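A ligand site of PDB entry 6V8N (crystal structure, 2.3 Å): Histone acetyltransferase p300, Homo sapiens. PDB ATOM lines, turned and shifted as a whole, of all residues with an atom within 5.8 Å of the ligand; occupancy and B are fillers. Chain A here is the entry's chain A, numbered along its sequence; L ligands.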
ATOM      1  N   PHE A  89       9.996 -11.222 -27.153  1.00  0.00           N
ATOM      2  CA  PHE A  89       9.933 -10.326 -25.966  1.00  0.00           C
ATOM      3  C   PHE A  89       9.557 -11.090 -24.690  1.00  0.00           C
ATOM      4  O   PHE A  89       8.792 -12.032 -24.719  1.00  0.00           O
ATOM      5  CB  PHE A  89       8.951  -9.180 -26.218  1.00  0.00           C
ATOM      6  CG  PHE A  89       8.732  -8.296 -25.028  1.00  0.00           C
ATOM      7  CD1 PHE A  89       9.481  -7.152 -24.858  1.00  0.00           C
ATOM      8  CD2 PHE A  89       7.748  -8.596 -24.095  1.00  0.00           C
ATOM      9  CE1 PHE A  89       9.266  -6.326 -23.765  1.00  0.00           C
ATOM     10  CE2 PHE A  89       7.530  -7.782 -22.995  1.00  0.00           C
ATOM     11  CZ  PHE A  89       8.287  -6.658 -22.828  1.00  0.00           C
ATOM     12  N   LEU A 113      13.374  -6.879 -18.461  1.00  0.00           N
ATOM     13  CA  LEU A 113      12.798  -7.198 -19.781  1.00  0.00           C
ATOM     14  C   LEU A 113      13.920  -7.562 -20.740  1.00  0.00           C
ATOM     15  O   LEU A 113      15.116  -7.352 -20.453  1.00  0.00           O
ATOM     16  CB  LEU A 113      11.888  -6.081 -20.299  1.00  0.00           C
ATOM     17  CG  LEU A 113      12.390  -4.660 -20.181  1.00  0.00           C
ATOM     18  CD1 LEU A 113      13.426  -4.394 -21.237  1.00  0.00           C
ATOM     19  CD2 LEU A 113      11.226  -3.694 -20.298  1.00  0.00           C
ATOM     20  N   ASP A 114      13.521  -8.234 -21.811  1.00  0.00           N
ATOM     21  CA  ASP A 114      14.445  -8.707 -22.863  1.00  0.00           C
ATOM     22  C   ASP A 114      13.693  -8.850 -24.181  1.00  0.00           C
ATOM     23  O   ASP A 114      12.457  -8.893 -24.183  1.00  0.00           O
ATOM     24  CB  ASP A 114      15.144 -10.000 -22.460  1.00  0.00           C
ATOM     25  CG  ASP A 114      16.538 -10.120 -23.063  1.00  0.00           C
ATOM     26  OD1 ASP A 114      16.895  -9.287 -23.957  1.00  0.00           O
ATOM     27  OD2 ASP A 114      17.274 -11.073 -22.661  1.00  0.00           O
ATOM     28  N   SER A 115      14.470  -8.917 -25.253  1.00  0.00           N
ATOM     29  CA  SER A 115      13.957  -9.058 -26.631  1.00  0.00           C
ATOM     30  C   SER A 115      14.964  -9.784 -27.526  1.00  0.00           C
ATOM     31  O   SER A 115      16.172  -9.656 -27.288  1.00  0.00           O
ATOM     32  CB  SER A 115      13.646  -7.715 -27.196  1.00  0.00           C
ATOM     33  OG  SER A 115      14.847  -6.975 -27.400  1.00  0.00           O
ATOM     34  N   THR A 126       9.803  -1.239 -32.217  1.00  0.00           N
ATOM     35  CA  THR A 126       9.746  -0.269 -31.116  1.00  0.00           C
ATOM     36  C   THR A 126       8.293  -0.060 -30.726  1.00  0.00           C
ATOM     37  O   THR A 126       7.990  -0.253 -29.556  1.00  0.00           O
ATOM     38  CB  THR A 126      10.419   1.042 -31.493  1.00  0.00           C
ATOM     39  OG1 THR A 126      11.808   0.702 -31.486  1.00  0.00           O
ATOM     40  CG2 THR A 126      10.128   2.133 -30.489  1.00  0.00           C
ATOM     41  N   TYR A 129       6.745  -3.056 -28.845  1.00  0.00           N
ATOM     42  CA  TYR A 129       7.316  -3.145 -27.468  1.00  0.00           C
ATOM     43  C   TYR A 129       6.559  -2.148 -26.597  1.00  0.00           C
ATOM     44  O   TYR A 129       6.178  -2.508 -25.485  1.00  0.00           O
ATOM     45  CB  TYR A 129       8.826  -2.872 -27.378  1.00  0.00           C
ATOM     46  CG  TYR A 129       9.746  -3.839 -28.078  1.00  0.00           C
ATOM     47  CD1 TYR A 129       9.537  -5.203 -28.039  1.00  0.00           C
ATOM     48  CD2 TYR A 129      10.867  -3.371 -28.737  1.00  0.00           C
ATOM     49  CE1 TYR A 129      10.405  -6.078 -28.686  1.00  0.00           C
ATOM     50  CE2 TYR A 129      11.738  -4.234 -29.391  1.00  0.00           C
ATOM     51  CZ  TYR A 129      11.494  -5.588 -29.379  1.00  0.00           C
ATOM     52  OH  TYR A 129      12.336  -6.438 -30.037  1.00  0.00           O
ATOM     53  N   LEU A 133       4.221  -2.679 -22.994  1.00  0.00           N
ATOM     54  CA  LEU A 133       4.534  -2.055 -21.681  1.00  0.00           C
ATOM     55  C   LEU A 133       3.411  -1.098 -21.295  1.00  0.00           C
ATOM     56  O   LEU A 133       3.017  -1.107 -20.132  1.00  0.00           O
ATOM     57  CB  LEU A 133       5.890  -1.338 -21.750  1.00  0.00           C
ATOM     58  CG  LEU A 133       7.085  -2.255 -21.909  1.00  0.00           C
ATOM     59  CD1 LEU A 133       8.344  -1.445 -22.156  1.00  0.00           C
ATOM     60  CD2 LEU A 133       7.271  -3.113 -20.673  1.00  0.00           C
ATOM     61  N   CYS A 153      18.455   0.178 -17.267  1.00  0.00           N
ATOM     62  CA  CYS A 153      19.764  -0.454 -17.034  1.00  0.00           C
ATOM     63  C   CYS A 153      19.948  -1.543 -18.062  1.00  0.00           C
ATOM     64  O   CYS A 153      19.321  -2.594 -18.022  1.00  0.00           O
ATOM     65  CB  CYS A 153      19.907  -1.059 -15.651  1.00  0.00           C
ATOM     66  SG  CYS A 153      21.621  -1.588 -15.383  1.00  0.00           S
ATOM     67  N   PRO A 154      20.806  -1.293 -19.057  1.00  0.00           N
ATOM     68  CA  PRO A 154      21.018  -2.283 -20.074  1.00  0.00           C
ATOM     69  C   PRO A 154      21.951  -3.354 -19.541  1.00  0.00           C
ATOM     70  O   PRO A 154      22.804  -3.130 -18.675  1.00  0.00           O
ATOM     71  CB  PRO A 154      21.676  -1.489 -21.205  1.00  0.00           C
ATOM     72  CG  PRO A 154      22.377  -0.354 -20.509  1.00  0.00           C
ATOM     73  CD  PRO A 154      21.561  -0.059 -19.275  1.00  0.00           C
ATOM     74  N   PRO A 155      21.824  -4.532 -20.155  1.00  0.00           N
ATOM     75  CA  PRO A 155      22.786  -5.593 -19.908  1.00  0.00           C
ATOM     76  C   PRO A 155      24.215  -5.137 -20.224  1.00  0.00           C
ATOM     77  O   PRO A 155      24.419  -4.351 -21.145  1.00  0.00           O
ATOM     78  CB  PRO A 155      22.319  -6.730 -20.845  1.00  0.00           C
ATOM     79  CG  PRO A 155      21.332  -6.104 -21.807  1.00  0.00           C
ATOM     80  CD  PRO A 155      20.838  -4.805 -21.201  1.00  0.00           C
ATOM     81  N   SER A 156      25.189  -5.678 -19.508  1.00  0.00           N
ATOM     82  CA  SER A 156      26.641  -5.603 -19.839  1.00  0.00           C
ATOM     83  C   SER A 156      26.881  -6.284 -21.175  1.00  0.00           C
ATOM     84  O   SER A 156      26.103  -7.263 -21.459  1.00  0.00           O
ATOM     85  CB  SER A 156      27.480  -6.295 -18.790  1.00  0.00           C
ATOM     86  OG  SER A 156      27.274  -5.711 -17.523  1.00  0.00           O
ATOM     87  N   GLU A 157      27.970  -5.906 -21.875  1.00  0.00           N
ATOM     88  CA  GLU A 157      28.453  -6.551 -23.124  1.00  0.00           C
ATOM     89  C   GLU A 157      28.461  -8.072 -22.927  1.00  0.00           C
ATOM     90  O   GLU A 157      28.884  -8.535 -21.834  1.00  0.00           O
ATOM     91  CB  GLU A 157      29.843  -6.041 -23.521  1.00  0.00           C
ATOM     92  N   GLY A 158      27.900  -8.814 -23.894  1.00  0.00           N
ATOM     93  CA  GLY A 158      27.900 -10.292 -23.940  1.00  0.00           C
ATOM     94  C   GLY A 158      26.893 -10.947 -22.984  1.00  0.00           C
ATOM     95  O   GLY A 158      26.594 -12.151 -23.223  1.00  0.00           O
ATOM     96  N   ASP A 159      26.383 -10.230 -21.966  1.00  0.00           N
ATOM     97  CA  ASP A 159      25.446 -10.783 -20.947  1.00  0.00           C
ATOM     98  C   ASP A 159      23.997 -10.786 -21.495  1.00  0.00           C
ATOM     99  O   ASP A 159      23.698 -10.029 -22.434  1.00  0.00           O
ATOM    100  CB  ASP A 159      25.557 -10.014 -19.623  1.00  0.00           C
ATOM    101  CG  ASP A 159      24.938 -10.739 -18.446  1.00  0.00           C
ATOM    102  OD1 ASP A 159      25.333 -11.912 -18.200  1.00  0.00           O
ATOM    103  OD2 ASP A 159      24.022 -10.147 -17.817  1.00  0.00           O
ATOM    104  N   ASP A 160      23.131 -11.637 -20.934  1.00  0.00           N
ATOM    105  CA  ASP A 160      21.770 -11.940 -21.419  1.00  0.00           C
ATOM    106  C   ASP A 160      20.842 -11.879 -20.216  1.00  0.00           C
ATOM    107  O   ASP A 160      21.084 -12.619 -19.286  1.00  0.00           O
ATOM    108  CB  ASP A 160      21.663 -13.346 -22.001  1.00  0.00           C
ATOM    109  CG  ASP A 160      22.459 -13.619 -23.277  1.00  0.00           C
ATOM    110  OD1 ASP A 160      22.495 -12.709 -24.164  1.00  0.00           O
ATOM    111  OD2 ASP A 160      22.972 -14.758 -23.385  1.00  0.00           O
ATOM    112  N   TYR A 161      19.851 -11.004 -20.220  1.00  0.00           N
ATOM    113  CA  TYR A 161      18.871 -10.918 -19.097  1.00  0.00           C
ATOM    114  C   TYR A 161      17.915 -12.125 -19.140  1.00  0.00           C
ATOM    115  O   TYR A 161      17.713 -12.693 -18.060  1.00  0.00           O
ATOM    116  CB  TYR A 161      18.070  -9.610 -19.098  1.00  0.00           C
ATOM    117  CG  TYR A 161      18.743  -8.379 -18.565  1.00  0.00           C
ATOM    118  CD1 TYR A 161      19.951  -8.404 -17.858  1.00  0.00           C
ATOM    119  CD2 TYR A 161      18.145  -7.142 -18.738  1.00  0.00           C
ATOM    120  CE1 TYR A 161      20.542  -7.242 -17.361  1.00  0.00           C
ATOM    121  CE2 TYR A 161      18.723  -5.971 -18.273  1.00  0.00           C
ATOM    122  CZ  TYR A 161      19.920  -6.013 -17.573  1.00  0.00           C
ATOM    123  OH  TYR A 161      20.416  -4.829 -17.103  1.00  0.00           O
ATOM    124  N   HIS A 166      22.228 -13.781 -27.793  1.00  0.00           N
ATOM    125  CA  HIS A 166      21.525 -12.849 -28.720  1.00  0.00           C
ATOM    126  C   HIS A 166      22.278 -12.802 -30.064  1.00  0.00           C
ATOM    127  O   HIS A 166      23.438 -13.230 -30.143  1.00  0.00           O
ATOM    128  CB  HIS A 166      21.393 -11.455 -28.080  1.00  0.00           C
ATOM    129  CG  HIS A 166      20.349 -11.318 -27.022  1.00  0.00           C
ATOM    130  ND1 HIS A 166      20.532 -11.818 -25.730  1.00  0.00           N
ATOM    131  CD2 HIS A 166      19.149 -10.696 -27.042  1.00  0.00           C
ATOM    132  CE1 HIS A 166      19.452 -11.529 -25.013  1.00  0.00           C
ATOM    133  NE2 HIS A 166      18.589 -10.843 -25.794  1.00  0.00           N
ATOM    134  N   PRO A 167      21.643 -12.297 -31.154  1.00  0.00           N
ATOM    135  CA  PRO A 167      22.324 -12.129 -32.432  1.00  0.00           C
ATOM    136  C   PRO A 167      23.521 -11.176 -32.300  1.00  0.00           C
ATOM    137  O   PRO A 167      23.456 -10.196 -31.557  1.00  0.00           O
ATOM    138  CB  PRO A 167      21.260 -11.551 -33.392  1.00  0.00           C
ATOM    139  CG  PRO A 167      19.942 -11.928 -32.724  1.00  0.00           C
ATOM    140  CD  PRO A 167      20.226 -11.895 -31.236  1.00  0.00           C
ATOM    141  N   PRO A 168      24.648 -11.503 -32.963  1.00  0.00           N
ATOM    142  CA  PRO A 168      25.845 -10.656 -32.941  1.00  0.00           C
ATOM    143  C   PRO A 168      25.591  -9.189 -33.315  1.00  0.00           C
ATOM    144  O   PRO A 168      26.300  -8.319 -32.799  1.00  0.00           O
ATOM    145  CB  PRO A 168      26.808 -11.292 -33.972  1.00  0.00           C
ATOM    146  CG  PRO A 168      26.272 -12.717 -34.225  1.00  0.00           C
ATOM    147  CD  PRO A 168      24.860 -12.778 -33.681  1.00  0.00           C
ATOM    148  N   GLN A 170      22.533  -7.631 -32.988  1.00  0.00           N
ATOM    149  CA  GLN A 170      21.581  -6.963 -32.042  1.00  0.00           C
ATOM    150  C   GLN A 170      22.417  -6.203 -31.006  1.00  0.00           C
ATOM    151  O   GLN A 170      22.994  -6.860 -30.115  1.00  0.00           O
ATOM    152  CB  GLN A 170      20.592  -7.908 -31.332  1.00  0.00           C
ATOM    153  CG  GLN A 170      19.551  -7.114 -30.534  1.00  0.00           C
ATOM    154  CD  GLN A 170      18.541  -7.983 -29.831  1.00  0.00           C
ATOM    155  OE1 GLN A 170      18.285  -9.114 -30.243  1.00  0.00           O
ATOM    156  NE2 GLN A 170      17.975  -7.466 -28.748  1.00  0.00           N
ATOM    157  N   LYS A 171      22.431  -4.874 -31.109  1.00  0.00           N
ATOM    158  CA  LYS A 171      23.292  -3.979 -30.319  1.00  0.00           C
ATOM    159  C   LYS A 171      22.582  -3.662 -28.992  1.00  0.00           C
ATOM    160  O   LYS A 171      21.339  -3.546 -28.925  1.00  0.00           O
ATOM    161  CB  LYS A 171      23.647  -2.733 -31.134  1.00  0.00           C
ATOM    162  CG  LYS A 171      24.273  -2.989 -32.519  1.00  0.00           C
ATOM    163  CD  LYS A 171      25.659  -3.592 -32.493  1.00  0.00           C
ATOM    164  CE  LYS A 171      26.703  -2.650 -31.924  1.00  0.00           C
ATOM    165  NZ  LYS A 171      28.055  -3.254 -31.928  1.00  0.00           N
ATOM    166  N   ILE A 172      23.373  -3.556 -27.937  1.00  0.00           N
ATOM    167  CA  ILE A 172      22.858  -3.108 -26.638  1.00  0.00           C
ATOM    168  C   ILE A 172      22.758  -1.608 -26.694  1.00  0.00           C
ATOM    169  O   ILE A 172      23.775  -0.948 -26.791  1.00  0.00           O
ATOM    170  CB  ILE A 172      23.750  -3.546 -25.462  1.00  0.00           C
ATOM    171  CG1 ILE A 172      23.817  -5.077 -25.358  1.00  0.00           C
ATOM    172  CG2 ILE A 172      23.221  -2.913 -24.194  1.00  0.00           C
ATOM    173  CD1 ILE A 172      24.920  -5.594 -24.406  1.00  0.00           C
ATOM    174  N   PRO A 173      21.579  -1.020 -26.390  1.00  0.00           N
ATOM    175  CA  PRO A 173      21.515   0.427 -26.249  1.00  0.00           C
ATOM    176  C   PRO A 173      22.444   0.917 -25.111  1.00  0.00           C
ATOM    177  O   PRO A 173      22.584   0.262 -24.089  1.00  0.00           O
ATOM    178  CB  PRO A 173      20.028   0.714 -25.954  1.00  0.00           C
ATOM    179  CG  PRO A 173      19.464  -0.593 -25.456  1.00  0.00           C
ATOM    180  CD  PRO A 173      20.316  -1.689 -26.045  1.00  0.00           C
ATOM    181  N   ARG A 177      20.296   6.605 -24.749  1.00  0.00           N
ATOM    182  CA  ARG A 177      19.341   6.077 -25.734  1.00  0.00           C
ATOM    183  C   ARG A 177      18.233   5.334 -24.981  1.00  0.00           C
ATOM    184  O   ARG A 177      17.061   5.610 -25.228  1.00  0.00           O
ATOM    185  CB  ARG A 177      20.087   5.188 -26.741  1.00  0.00           C
ATOM    186  CG  ARG A 177      19.172   4.479 -27.718  1.00  0.00           C
ATOM    187  CD  ARG A 177      20.007   3.927 -28.885  1.00  0.00           C
ATOM    188  NE  ARG A 177      19.336   2.782 -29.428  1.00  0.00           N
ATOM    189  CZ  ARG A 177      18.286   2.835 -30.239  1.00  0.00           C
ATOM    190  NH1 ARG A 177      17.847   4.007 -30.675  1.00  0.00           N
ATOM    191  NH2 ARG A 177      17.708   1.716 -30.627  1.00  0.00           N
ATOM    192  N   LEU A 178      18.581   4.453 -24.051  1.00  0.00           N
ATOM    193  CA  LEU A 178      17.567   3.651 -23.291  1.00  0.00           C
ATOM    194  C   LEU A 178      16.689   4.584 -22.463  1.00  0.00           C
ATOM    195  O   LEU A 178      15.498   4.411 -22.455  1.00  0.00           O
ATOM    196  CB  LEU A 178      18.274   2.648 -22.370  1.00  0.00           C
ATOM    197  CG  LEU A 178      17.362   1.728 -21.573  1.00  0.00           C
ATOM    198  CD1 LEU A 178      16.419   0.983 -22.482  1.00  0.00           C
ATOM    199  CD2 LEU A 178      18.174   0.754 -20.748  1.00  0.00           C
ATOM    200  N   TRP A 181      14.291   6.143 -24.800  1.00  0.00           N
ATOM    201  CA  TRP A 181      13.330   5.118 -25.223  1.00  0.00           C
ATOM    202  C   TRP A 181      12.225   4.988 -24.160  1.00  0.00           C
ATOM    203  O   TRP A 181      11.053   4.923 -24.490  1.00  0.00           O
ATOM    204  CB  TRP A 181      14.094   3.826 -25.437  1.00  0.00           C
ATOM    205  CG  TRP A 181      13.336   2.703 -26.047  1.00  0.00           C
ATOM    206  CD1 TRP A 181      13.368   2.327 -27.357  1.00  0.00           C
ATOM    207  CD2 TRP A 181      12.540   1.728 -25.342  1.00  0.00           C
ATOM    208  NE1 TRP A 181      12.644   1.174 -27.502  1.00  0.00           N
ATOM    209  CE2 TRP A 181      12.128   0.787 -26.292  1.00  0.00           C
ATOM    210  CE3 TRP A 181      12.144   1.550 -24.011  1.00  0.00           C
ATOM    211  CZ2 TRP A 181      11.317  -0.304 -25.978  1.00  0.00           C
ATOM    212  CZ3 TRP A 181      11.345   0.487 -23.687  1.00  0.00           C
ATOM    213  CH2 TRP A 181      10.948  -0.440 -24.651  1.00  0.00           C
ATOM    214  N   TYR A 182      12.563   4.910 -22.897  1.00  0.00           N
ATOM    215  CA  TYR A 182      11.508   4.815 -21.857  1.00  0.00           C
ATOM    216  C   TYR A 182      10.693   6.119 -21.841  1.00  0.00           C
ATOM    217  O   TYR A 182       9.462   6.061 -21.624  1.00  0.00           O
ATOM    218  CB  TYR A 182      12.146   4.487 -20.491  1.00  0.00           C
ATOM    219  CG  TYR A 182      12.516   3.051 -20.262  1.00  0.00           C
ATOM    220  CD1 TYR A 182      11.543   2.073 -20.147  1.00  0.00           C
ATOM    221  CD2 TYR A 182      13.840   2.648 -20.075  1.00  0.00           C
ATOM    222  CE1 TYR A 182      11.864   0.742 -19.872  1.00  0.00           C
ATOM    223  CE2 TYR A 182      14.176   1.319 -19.774  1.00  0.00           C
ATOM    224  CZ  TYR A 182      13.183   0.361 -19.649  1.00  0.00           C
ATOM    225  OH  TYR A 182      13.471  -0.952 -19.356  1.00  0.00           O
HETATM  226  C1  LIG L   1      14.246  -1.994 -25.049  1.00  0.00           C
HETATM  227  C2  LIG L   1      16.924  -4.412 -21.179  1.00  0.00           C
HETATM  228  C3  LIG L   1      14.842  -0.788 -25.205  1.00  0.00           C
HETATM  229  C4  LIG L   1      15.415  -0.455 -26.415  1.00  0.00           C
HETATM  230  C5  LIG L   1      16.855  -5.765 -24.726  1.00  0.00           C
HETATM  231  C6  LIG L   1      16.056   0.817 -26.555  1.00  0.00           C
HETATM  232  C7  LIG L   1      15.380  -1.347 -27.476  1.00  0.00           C
HETATM  233  C8  LIG L   1      14.766  -2.579 -27.299  1.00  0.00           C
HETATM  234  C9  LIG L   1      14.431  -5.109 -24.969  1.00  0.00           C
HETATM  235  C10 LIG L   1      17.071  -4.845 -23.532  1.00  0.00           C
HETATM  236  C11 LIG L   1      16.754  -5.260 -22.261  1.00  0.00           C
HETATM  237  N1  LIG L   1      16.560   1.847 -26.607  1.00  0.00           N
HETATM  238  N2  LIG L   1      15.764  -5.234 -25.577  1.00  0.00           N
HETATM  239  C12 LIG L   1      14.175  -2.910 -26.093  1.00  0.00           C
HETATM  240  N3  LIG L   1      18.887  -7.014 -25.142  1.00  0.00           N
HETATM  241  C13 LIG L   1      12.125  -4.098 -25.246  1.00  0.00           C
HETATM  242  C14 LIG L   1      13.527  -4.248 -25.854  1.00  0.00           C
HETATM  243  C15 LIG L   1      17.364  -3.122 -21.382  1.00  0.00           C
HETATM  244  C16 LIG L   1      17.681  -2.698 -22.651  1.00  0.00           C
HETATM  245  C17 LIG L   1      17.529  -3.560 -23.722  1.00  0.00           C
HETATM  246  C18 LIG L   1      18.163  -5.942 -25.490  1.00  0.00           C
HETATM  247  C19 LIG L   1      20.139  -7.447 -25.623  1.00  0.00           C
HETATM  248  N4  LIG L   1      20.745  -8.283 -24.769  1.00  0.00           N
HETATM  249  C20 LIG L   1      21.931  -8.788 -25.115  1.00  0.00           C
HETATM  250  C21 LIG L   1      22.579  -8.466 -26.300  1.00  0.00           C
HETATM  251  C22 LIG L   1      23.860  -9.114 -26.637  1.00  0.00           C
HETATM  252  C23 LIG L   1      24.454  -9.115 -27.882  1.00  0.00           C
HETATM  253  N5  LIG L   1      25.547  -9.907 -27.781  1.00  0.00           N
HETATM  254  C24 LIG L   1      26.543 -10.218 -28.797  1.00  0.00           C
HETATM  255  N6  LIG L   1      25.681 -10.448 -26.521  1.00  0.00           N
HETATM  256  C25 LIG L   1      24.640  -9.975 -25.844  1.00  0.00           C
HETATM  257  C26 LIG L   1      21.919  -7.620 -27.184  1.00  0.00           C
HETATM  258  C27 LIG L   1      20.688  -7.087 -26.853  1.00  0.00           C
HETATM  259  O1  LIG L   1      18.491  -5.136 -26.356  1.00  0.00           O
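Phe 89 touches the ligand.
Leu 113 touches the ligand (O to C11, 3.2 Å).
Tyr 129 touches the ligand.
O of Cys 153 touches C15 of the ligand, 3.9 Å away.
Pro 154 touches the ligand.
Pro 155 touches the ligand (CG to N4, 3.7 Å).
Gly 158 touches the ligand.
O of Asp 159 touches C20 of the ligand, at 3.4 Å.
OD1 of Asp 160 touches C25 of the ligand, at 3.9 Å.
CE2 of Tyr 161 touches C2 of the ligand, 3.8 Å away.
His 166 touches the ligand (ND1 to C20, 3.4 Å).
Pro 167 touches the ligand (O to C23, 3.96 Å).
CG1 of Ile 172 touches C26 of the ligand (3.7 Å).
Pro 173 touches the ligand.
CG of Arg 177 touches N1 of the ligand, at 3.9 Å.
Leu 178 touches the ligand (CD1 to C3, 3.6 Å).
Trp 181 touches the ligand.
Hydrophobic or aromatic side chains that line the ligand: Phe 89, Leu 113, Tyr 129, Pro 155, Tyr 161, His 166, Ile 172, Pro 173, Leu 178 and Trp 181.
Of the 27 residues printed, 20 come within 4 Å of the ligand.
Along chain A the residues within 4 Å of the ligand span positions 89 to 181.
The side-chain hydroxyl of Tyr 161 lies close to the backbone carbonyl oxygen of Pro 154 (3.3 Å).
OD1 of Asp 114 lies within hydrogen-bond range of NE2 of His 166 (2.9 Å).
The side-chain carboxylate of Asp 160 sits at hydrogen-bond distance from a ring nitrogen (ND1) of His 166 (2.7 Å).
The side-chain hydroxyl of Tyr 161 is in hydrogen-bond range of the backbone carbonyl oxygen of Cys 153, 2.7 Å away.
The side-chain amide nitrogen of Gln 170 lies within hydrogen-bond range of the backbone carbonyl oxygen of Ser 115, at 3.2 Å.
The backbone carbonyl oxygen of Ser 115 sits at hydrogen-bond distance from a ring nitrogen (NE2) of His 166, 3.1 Å away.
The side-chain amide nitrogen (NE2) of Gln 170 sits close to an oxygen (O1) of the ligand (3.4 Å).
The side-chain carboxylate (OD1) of Asp 114 is in hydrogen-bond range of a nitrogen (N3) of the ligand (3.2 Å).
The side-chain hydroxyl of Ser 115 lies within hydrogen-bond range of a nitrogen (N2) of the ligand.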
